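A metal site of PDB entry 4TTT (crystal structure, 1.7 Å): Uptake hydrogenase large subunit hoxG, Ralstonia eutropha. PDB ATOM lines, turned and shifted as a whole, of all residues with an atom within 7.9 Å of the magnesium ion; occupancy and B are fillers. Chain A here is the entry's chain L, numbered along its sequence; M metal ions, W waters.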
ATOM      1  N   TRP A  52     -20.439   7.151   5.872  1.00  0.00           N
ATOM      2  CA  TRP A  52     -19.457   7.644   4.924  1.00  0.00           C
ATOM      3  C   TRP A  52     -19.302   9.144   5.125  1.00  0.00           C
ATOM      4  O   TRP A  52     -20.284   9.828   5.418  1.00  0.00           O
ATOM      5  CB  TRP A  52     -19.883   7.322   3.488  1.00  0.00           C
ATOM      6  CG  TRP A  52     -18.939   7.832   2.440  1.00  0.00           C
ATOM      7  CD1 TRP A  52     -17.656   7.421   2.222  1.00  0.00           C
ATOM      8  CD2 TRP A  52     -19.199   8.849   1.465  1.00  0.00           C
ATOM      9  NE1 TRP A  52     -17.110   8.112   1.162  1.00  0.00           N
ATOM     10  CE2 TRP A  52     -18.031   8.999   0.688  1.00  0.00           C
ATOM     11  CE3 TRP A  52     -20.309   9.653   1.177  1.00  0.00           C
ATOM     12  CZ2 TRP A  52     -17.945   9.921  -0.362  1.00  0.00           C
ATOM     13  CZ3 TRP A  52     -20.226  10.570   0.139  1.00  0.00           C
ATOM     14  CH2 TRP A  52     -19.044  10.703  -0.615  1.00  0.00           C
ATOM     15  N   GLU A  56     -11.669  11.280   0.775  1.00  0.00           N
ATOM     16  CA  GLU A  56     -10.965  11.209  -0.512  1.00  0.00           C
ATOM     17  C   GLU A  56     -11.399  12.347  -1.445  1.00  0.00           C
ATOM     18  O   GLU A  56     -10.585  12.895  -2.200  1.00  0.00           O
ATOM     19  CB  GLU A  56     -11.196   9.851  -1.147  1.00  0.00           C
ATOM     20  CG  GLU A  56     -10.514   8.714  -0.379  1.00  0.00           C
ATOM     21  CD  GLU A  56     -11.107   7.351  -0.635  1.00  0.00           C
ATOM     22  OE1 GLU A  56     -12.292   7.273  -1.029  1.00  0.00           O
ATOM     23  OE2 GLU A  56     -10.389   6.348  -0.426  1.00  0.00           O
ATOM     24  N   ILE A  74      -9.643  10.570   9.751  1.00  0.00           N
ATOM     25  CA  ILE A  74     -10.390   9.358   9.415  1.00  0.00           C
ATOM     26  C   ILE A  74     -10.770   8.607  10.691  1.00  0.00           C
ATOM     27  O   ILE A  74     -11.867   8.044  10.781  1.00  0.00           O
ATOM     28  CB  ILE A  74      -9.597   8.444   8.457  1.00  0.00           C
ATOM     29  CG1 ILE A  74      -9.599   9.071   7.062  1.00  0.00           C
ATOM     30  CG2 ILE A  74     -10.211   7.045   8.385  1.00  0.00           C
ATOM     31  CD1 ILE A  74      -8.698   8.377   6.064  1.00  0.00           C
ATOM     32  N   GLU A 347      -9.944  -2.416  -5.853  1.00  0.00           N
ATOM     33  CA  GLU A 347     -11.209  -2.276  -5.147  1.00  0.00           C
ATOM     34  C   GLU A 347     -12.383  -2.319  -6.100  1.00  0.00           C
ATOM     35  O   GLU A 347     -12.408  -1.568  -7.095  1.00  0.00           O
ATOM     36  CB  GLU A 347     -11.249  -0.969  -4.387  1.00  0.00           C
ATOM     37  CG  GLU A 347     -10.281  -0.892  -3.220  1.00  0.00           C
ATOM     38  CD  GLU A 347     -10.442   0.395  -2.457  1.00  0.00           C
ATOM     39  OE1 GLU A 347     -10.132   1.468  -3.030  1.00  0.00           O
ATOM     40  OE2 GLU A 347     -10.879   0.343  -1.285  1.00  0.00           O
ATOM     41  N   TYR A 354     -21.281   3.071  -4.386  1.00  0.00           N
ATOM     42  CA  TYR A 354     -20.462   3.944  -5.224  1.00  0.00           C
ATOM     43  C   TYR A 354     -20.707   3.576  -6.690  1.00  0.00           C
ATOM     44  O   TYR A 354     -21.378   2.585  -6.983  1.00  0.00           O
ATOM     45  CB  TYR A 354     -18.967   3.791  -4.885  1.00  0.00           C
ATOM     46  CG  TYR A 354     -18.646   4.032  -3.446  1.00  0.00           C
ATOM     47  CD1 TYR A 354     -18.479   5.322  -2.948  1.00  0.00           C
ATOM     48  CD2 TYR A 354     -18.500   2.974  -2.551  1.00  0.00           C
ATOM     49  CE1 TYR A 354     -18.188   5.553  -1.615  1.00  0.00           C
ATOM     50  CE2 TYR A 354     -18.206   3.181  -1.217  1.00  0.00           C
ATOM     51  CZ  TYR A 354     -18.063   4.491  -0.750  1.00  0.00           C
ATOM     52  OH  TYR A 354     -17.784   4.733   0.567  1.00  0.00           O
ATOM     53  N   PRO A 365      -5.670   1.694  -6.474  1.00  0.00           N
ATOM     54  CA  PRO A 365      -6.016   2.974  -5.855  1.00  0.00           C
ATOM     55  C   PRO A 365      -5.407   4.234  -6.484  1.00  0.00           C
ATOM     56  O   PRO A 365      -5.977   5.306  -6.314  1.00  0.00           O
ATOM     57  CB  PRO A 365      -5.585   2.806  -4.390  1.00  0.00           C
ATOM     58  CG  PRO A 365      -5.527   1.331  -4.176  1.00  0.00           C
ATOM     59  CD  PRO A 365      -5.085   0.762  -5.495  1.00  0.00           C
ATOM     60  N   GLY A 368      -8.166   5.074  -8.449  1.00  0.00           N
ATOM     61  CA  GLY A 368      -9.394   4.906  -7.688  1.00  0.00           C
ATOM     62  C   GLY A 368     -10.370   6.051  -7.897  1.00  0.00           C
ATOM     63  O   GLY A 368      -9.968   7.166  -8.227  1.00  0.00           O
ATOM     64  N   VAL A 369     -11.653   5.737  -7.709  1.00  0.00           N
ATOM     65  CA  VAL A 369     -12.753   6.672  -7.910  1.00  0.00           C
ATOM     66  C   VAL A 369     -13.729   6.551  -6.739  1.00  0.00           C
ATOM     67  O   VAL A 369     -14.052   5.441  -6.314  1.00  0.00           O
ATOM     68  CB  VAL A 369     -13.501   6.379  -9.232  1.00  0.00           C
ATOM     69  CG1 VAL A 369     -14.735   7.252  -9.378  1.00  0.00           C
ATOM     70  CG2 VAL A 369     -12.561   6.565 -10.422  1.00  0.00           C
ATOM     71  N   THR A 370     -14.173   7.689  -6.222  1.00  0.00           N
ATOM     72  CA  THR A 370     -15.100   7.714  -5.080  1.00  0.00           C
ATOM     73  C   THR A 370     -16.261   8.659  -5.381  1.00  0.00           C
ATOM     74  O   THR A 370     -16.213   9.834  -5.059  1.00  0.00           O
ATOM     75  CB  THR A 370     -14.377   8.114  -3.776  1.00  0.00           C
ATOM     76  OG1 THR A 370     -13.270   7.230  -3.578  1.00  0.00           O
ATOM     77  CG2 THR A 370     -15.304   8.025  -2.563  1.00  0.00           C
ATOM     78  N   TRP A 398     -21.369   1.065   2.528  1.00  0.00           N
ATOM     79  CA  TRP A 398     -20.487   2.192   2.231  1.00  0.00           C
ATOM     80  C   TRP A 398     -19.014   1.755   2.163  1.00  0.00           C
ATOM     81  O   TRP A 398     -18.151   2.580   1.898  1.00  0.00           O
ATOM     82  CB  TRP A 398     -20.663   3.314   3.260  1.00  0.00           C
ATOM     83  CG  TRP A 398     -21.917   4.121   3.085  1.00  0.00           C
ATOM     84  CD1 TRP A 398     -22.999   4.160   3.929  1.00  0.00           C
ATOM     85  CD2 TRP A 398     -22.225   5.014   2.014  1.00  0.00           C
ATOM     86  NE1 TRP A 398     -23.955   5.014   3.441  1.00  0.00           N
ATOM     87  CE2 TRP A 398     -23.510   5.553   2.267  1.00  0.00           C
ATOM     88  CE3 TRP A 398     -21.540   5.412   0.850  1.00  0.00           C
ATOM     89  CZ2 TRP A 398     -24.125   6.458   1.402  1.00  0.00           C
ATOM     90  CZ3 TRP A 398     -22.154   6.326  -0.004  1.00  0.00           C
ATOM     91  CH2 TRP A 398     -23.436   6.838   0.279  1.00  0.00           C
ATOM     92  N   LYS A 400     -16.063  -0.199   0.277  1.00  0.00           N
ATOM     93  CA  LYS A 400     -15.636  -0.802  -0.996  1.00  0.00           C
ATOM     94  C   LYS A 400     -15.139  -2.242  -0.753  1.00  0.00           C
ATOM     95  O   LYS A 400     -14.993  -2.668   0.389  1.00  0.00           O
ATOM     96  CB  LYS A 400     -14.522   0.033  -1.640  1.00  0.00           C
ATOM     97  CG  LYS A 400     -14.905   1.452  -2.042  1.00  0.00           C
ATOM     98  CD  LYS A 400     -13.798   2.104  -2.860  1.00  0.00           C
ATOM     99  CE  LYS A 400     -14.216   3.475  -3.382  1.00  0.00           C
ATOM    100  NZ  LYS A 400     -13.048   4.297  -3.789  1.00  0.00           N
ATOM    101  N   PRO A 402     -11.980  -4.410  -1.391  1.00  0.00           N
ATOM    102  CA  PRO A 402     -10.607  -4.604  -1.833  1.00  0.00           C
ATOM    103  C   PRO A 402     -10.322  -6.094  -2.022  1.00  0.00           C
ATOM    104  O   PRO A 402     -10.793  -6.913  -1.231  1.00  0.00           O
ATOM    105  CB  PRO A 402      -9.766  -4.055  -0.668  1.00  0.00           C
ATOM    106  CG  PRO A 402     -10.734  -3.376   0.249  1.00  0.00           C
ATOM    107  CD  PRO A 402     -12.029  -4.091   0.040  1.00  0.00           C
ATOM    108  N   GLY A 534      -3.038   1.367   3.329  1.00  0.00           N
ATOM    109  CA  GLY A 534      -2.342   2.049   2.249  1.00  0.00           C
ATOM    110  C   GLY A 534      -3.013   3.364   1.872  1.00  0.00           C
ATOM    111  O   GLY A 534      -4.238   3.440   1.822  1.00  0.00           O
ATOM    112  N   TRP A 536      -2.634   6.097  -1.386  1.00  0.00           N
ATOM    113  CA  TRP A 536      -2.103   6.303  -2.733  1.00  0.00           C
ATOM    114  C   TRP A 536      -2.435   7.728  -3.163  1.00  0.00           C
ATOM    115  O   TRP A 536      -3.604   8.126  -3.164  1.00  0.00           O
ATOM    116  CB  TRP A 536      -2.739   5.307  -3.701  1.00  0.00           C
ATOM    117  CG  TRP A 536      -2.239   3.893  -3.596  1.00  0.00           C
ATOM    118  CD1 TRP A 536      -1.334   3.291  -4.421  1.00  0.00           C
ATOM    119  CD2 TRP A 536      -2.661   2.891  -2.659  1.00  0.00           C
ATOM    120  NE1 TRP A 536      -1.145   1.976  -4.042  1.00  0.00           N
ATOM    121  CE2 TRP A 536      -1.946   1.713  -2.961  1.00  0.00           C
ATOM    122  CE3 TRP A 536      -3.572   2.876  -1.596  1.00  0.00           C
ATOM    123  CZ2 TRP A 536      -2.105   0.532  -2.230  1.00  0.00           C
ATOM    124  CZ3 TRP A 536      -3.724   1.700  -0.861  1.00  0.00           C
ATOM    125  CH2 TRP A 536      -3.001   0.547  -1.183  1.00  0.00           C
ATOM    126  N   TYR A 547      -6.449  11.111  -4.206  1.00  0.00           N
ATOM    127  CA  TYR A 547      -6.018  10.573  -2.929  1.00  0.00           C
ATOM    128  C   TYR A 547      -6.976   9.454  -2.576  1.00  0.00           C
ATOM    129  O   TYR A 547      -8.151   9.707  -2.356  1.00  0.00           O
ATOM    130  CB  TYR A 547      -5.995  11.653  -1.847  1.00  0.00           C
ATOM    131  CG  TYR A 547      -5.109  11.336  -0.661  1.00  0.00           C
ATOM    132  CD1 TYR A 547      -5.422  10.297   0.219  1.00  0.00           C
ATOM    133  CD2 TYR A 547      -3.936  12.072  -0.427  1.00  0.00           C
ATOM    134  CE1 TYR A 547      -4.599   9.998   1.300  1.00  0.00           C
ATOM    135  CE2 TYR A 547      -3.108  11.777   0.641  1.00  0.00           C
ATOM    136  CZ  TYR A 547      -3.447  10.747   1.508  1.00  0.00           C
ATOM    137  OH  TYR A 547      -2.615  10.457   2.562  1.00  0.00           O
ATOM    138  N   GLN A 548      -6.460   8.230  -2.549  1.00  0.00           N
ATOM    139  CA  GLN A 548      -7.275   7.058  -2.271  1.00  0.00           C
ATOM    140  C   GLN A 548      -6.681   6.272  -1.100  1.00  0.00           C
ATOM    141  O   GLN A 548      -5.480   6.003  -1.076  1.00  0.00           O
ATOM    142  CB  GLN A 548      -7.350   6.190  -3.530  1.00  0.00           C
ATOM    143  CG  GLN A 548      -8.185   6.813  -4.635  1.00  0.00           C
ATOM    144  CD  GLN A 548      -9.685   6.785  -4.338  1.00  0.00           C
ATOM    145  OE1 GLN A 548     -10.191   5.825  -3.793  1.00  0.00           O
ATOM    146  NE2 GLN A 548     -10.393   7.843  -4.736  1.00  0.00           N
ATOM    147  N   CYS A 549      -7.543   5.915  -0.154  1.00  0.00           N
ATOM    148  CA  CYS A 549      -7.184   5.113   1.003  1.00  0.00           C
ATOM    149  C   CYS A 549      -7.824   3.727   0.888  1.00  0.00           C
ATOM    150  O   CYS A 549      -9.002   3.605   0.536  1.00  0.00           O
ATOM    151  CB  CYS A 549      -7.677   5.798   2.292  1.00  0.00           C
ATOM    152  SG  CYS A 549      -7.114   7.498   2.514  1.00  0.00           S
ATOM    153  N   VAL A 550      -7.039   2.697   1.155  1.00  0.00           N
ATOM    154  CA  VAL A 550      -7.559   1.349   1.338  1.00  0.00           C
ATOM    155  C   VAL A 550      -7.116   0.939   2.747  1.00  0.00           C
ATOM    156  O   VAL A 550      -5.926   0.862   3.035  1.00  0.00           O
ATOM    157  CB  VAL A 550      -7.042   0.355   0.278  1.00  0.00           C
ATOM    158  CG1 VAL A 550      -7.816  -0.955   0.389  1.00  0.00           C
ATOM    159  CG2 VAL A 550      -7.217   0.921  -1.113  1.00  0.00           C
ATOM    160  N   VAL A 551      -8.102   0.711   3.607  1.00  0.00           N
ATOM    161  CA  VAL A 551      -7.899   0.694   5.054  1.00  0.00           C
ATOM    162  C   VAL A 551      -8.183  -0.735   5.569  1.00  0.00           C
ATOM    163  O   VAL A 551      -8.913  -1.482   4.922  1.00  0.00           O
ATOM    164  CB  VAL A 551      -8.791   1.801   5.674  1.00  0.00           C
ATOM    165  CG1 VAL A 551      -8.566   1.985   7.142  1.00  0.00           C
ATOM    166  CG2 VAL A 551      -8.573   3.131   4.966  1.00  0.00           C
ATOM    167  N   THR A 554     -11.639  -1.823   5.697  1.00  0.00           N
ATOM    168  CA  THR A 554     -12.157  -1.917   4.310  1.00  0.00           C
ATOM    169  C   THR A 554     -11.976  -3.358   3.781  1.00  0.00           C
ATOM    170  O   THR A 554     -12.911  -3.940   3.229  1.00  0.00           O
ATOM    171  CB  THR A 554     -11.470  -0.941   3.336  1.00  0.00           C
ATOM    172  OG1 THR A 554     -11.319   0.352   3.932  1.00  0.00           O
ATOM    173  CG2 THR A 554     -12.263  -0.819   2.057  1.00  0.00           C
ATOM    174  N   CYS A 600     -12.769   4.189   9.791  1.00  0.00           N
ATOM    175  CA  CYS A 600     -11.661   3.729   8.975  1.00  0.00           C
ATOM    176  C   CYS A 600     -12.105   3.066   7.689  1.00  0.00           C
ATOM    177  O   CYS A 600     -11.616   3.387   6.618  1.00  0.00           O
ATOM    178  CB  CYS A 600     -10.774   2.756   9.744  1.00  0.00           C
ATOM    179  SG  CYS A 600      -9.371   3.560  10.528  1.00  0.00           S
ATOM    180  N   SER A 601     -13.039   2.126   7.793  1.00  0.00           N
ATOM    181  CA  SER A 601     -13.403   1.303   6.640  1.00  0.00           C
ATOM    182  C   SER A 601     -13.954   2.128   5.488  1.00  0.00           C
ATOM    183  O   SER A 601     -13.760   1.773   4.329  1.00  0.00           O
ATOM    184  CB  SER A 601     -14.409   0.207   7.026  1.00  0.00           C
ATOM    185  OG  SER A 601     -15.687   0.743   7.272  1.00  0.00           O
ATOM    186  N   THR A 602     -14.623   3.231   5.824  1.00  0.00           N
ATOM    187  CA  THR A 602     -15.397   4.018   4.863  1.00  0.00           C
ATOM    188  C   THR A 602     -14.756   5.371   4.501  1.00  0.00           C
ATOM    189  O   THR A 602     -14.826   5.812   3.347  1.00  0.00           O
ATOM    190  CB  THR A 602     -16.818   4.253   5.414  1.00  0.00           C
ATOM    191  OG1 THR A 602     -16.738   4.862   6.703  1.00  0.00           O
ATOM    192  CG2 THR A 602     -17.588   2.927   5.537  1.00  0.00           C
ATOM    193  N   HIS A 603     -14.154   6.024   5.505  1.00  0.00           N
ATOM    194  CA  HIS A 603     -13.442   7.301   5.355  1.00  0.00           C
ATOM    195  C   HIS A 603     -14.162   8.293   4.426  1.00  0.00           C
ATOM    196  O   HIS A 603     -13.627   8.907   3.507  1.00  0.00           O
ATOM    197  CB  HIS A 603     -11.962   7.073   4.980  1.00  0.00           C
ATOM    198  CG  HIS A 603     -11.741   6.051   3.913  1.00  0.00           C
ATOM    199  ND1 HIS A 603     -11.693   4.695   4.188  1.00  0.00           N
ATOM    200  CD2 HIS A 603     -11.545   6.170   2.583  1.00  0.00           C
ATOM    201  CE1 HIS A 603     -11.486   4.025   3.066  1.00  0.00           C
ATOM    202  NE2 HIS A 603     -11.395   4.907   2.081  1.00  0.00           N
ATOM    203  OXT HIS A 603     -15.359   8.489   4.612  1.00  0.00           O
HETATM  204 MG    MG M   1     -10.959   4.221  -0.135  1.00  0.00          MG
HETATM  205  O   HOH W   1     -11.646   2.286   0.272  1.00  0.00           O
HETATM  206  O   HOH W   2     -12.952   4.723  -0.669  1.00  0.00           O
HETATM  207  O   HOH W   3     -10.469   3.833  -2.023  1.00  0.00           O
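The side-chain amide oxygen (OE1) of Gln 548 lies close to the side-chain carboxylate (OE2) of Glu 56, 3.4 Å away. OG1 of Thr 370 sits at hydrogen-bond distance from OE1 of Glu 56 (2.7 Å). ND1 of His 603 lies within hydrogen-bond range of O of Cys 600.
Water W3 binds the magnesium ion (2.0 Å). The magnesium ion is bound by water W1 (2.1 Å). The magnesium ion is bound by water W2 (2.1 Å). The backbone carbonyl oxygen (O) of Cys 549 is bound to the magnesium ion (2.2 Å). The magnesium ion is bound by the side-chain carboxylate (OE2) of Glu 56, 2.2 Å away. The magnesium ion is bound by NE2 of His 603.
Within 4 Å of the magnesium ion: Glu 56, Cys 549 and His 603.
Water W3 lies within hydrogen-bond range of OE1 of Glu 347 (2.6 Å), OE1 of Gln 548 (2.7 Å) and NZ of Lys 400 (3.2 Å). Water W2 bridges OE1 of Glu 56 (2.7 Å) and NZ of Lys 400 (3.2 Å).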
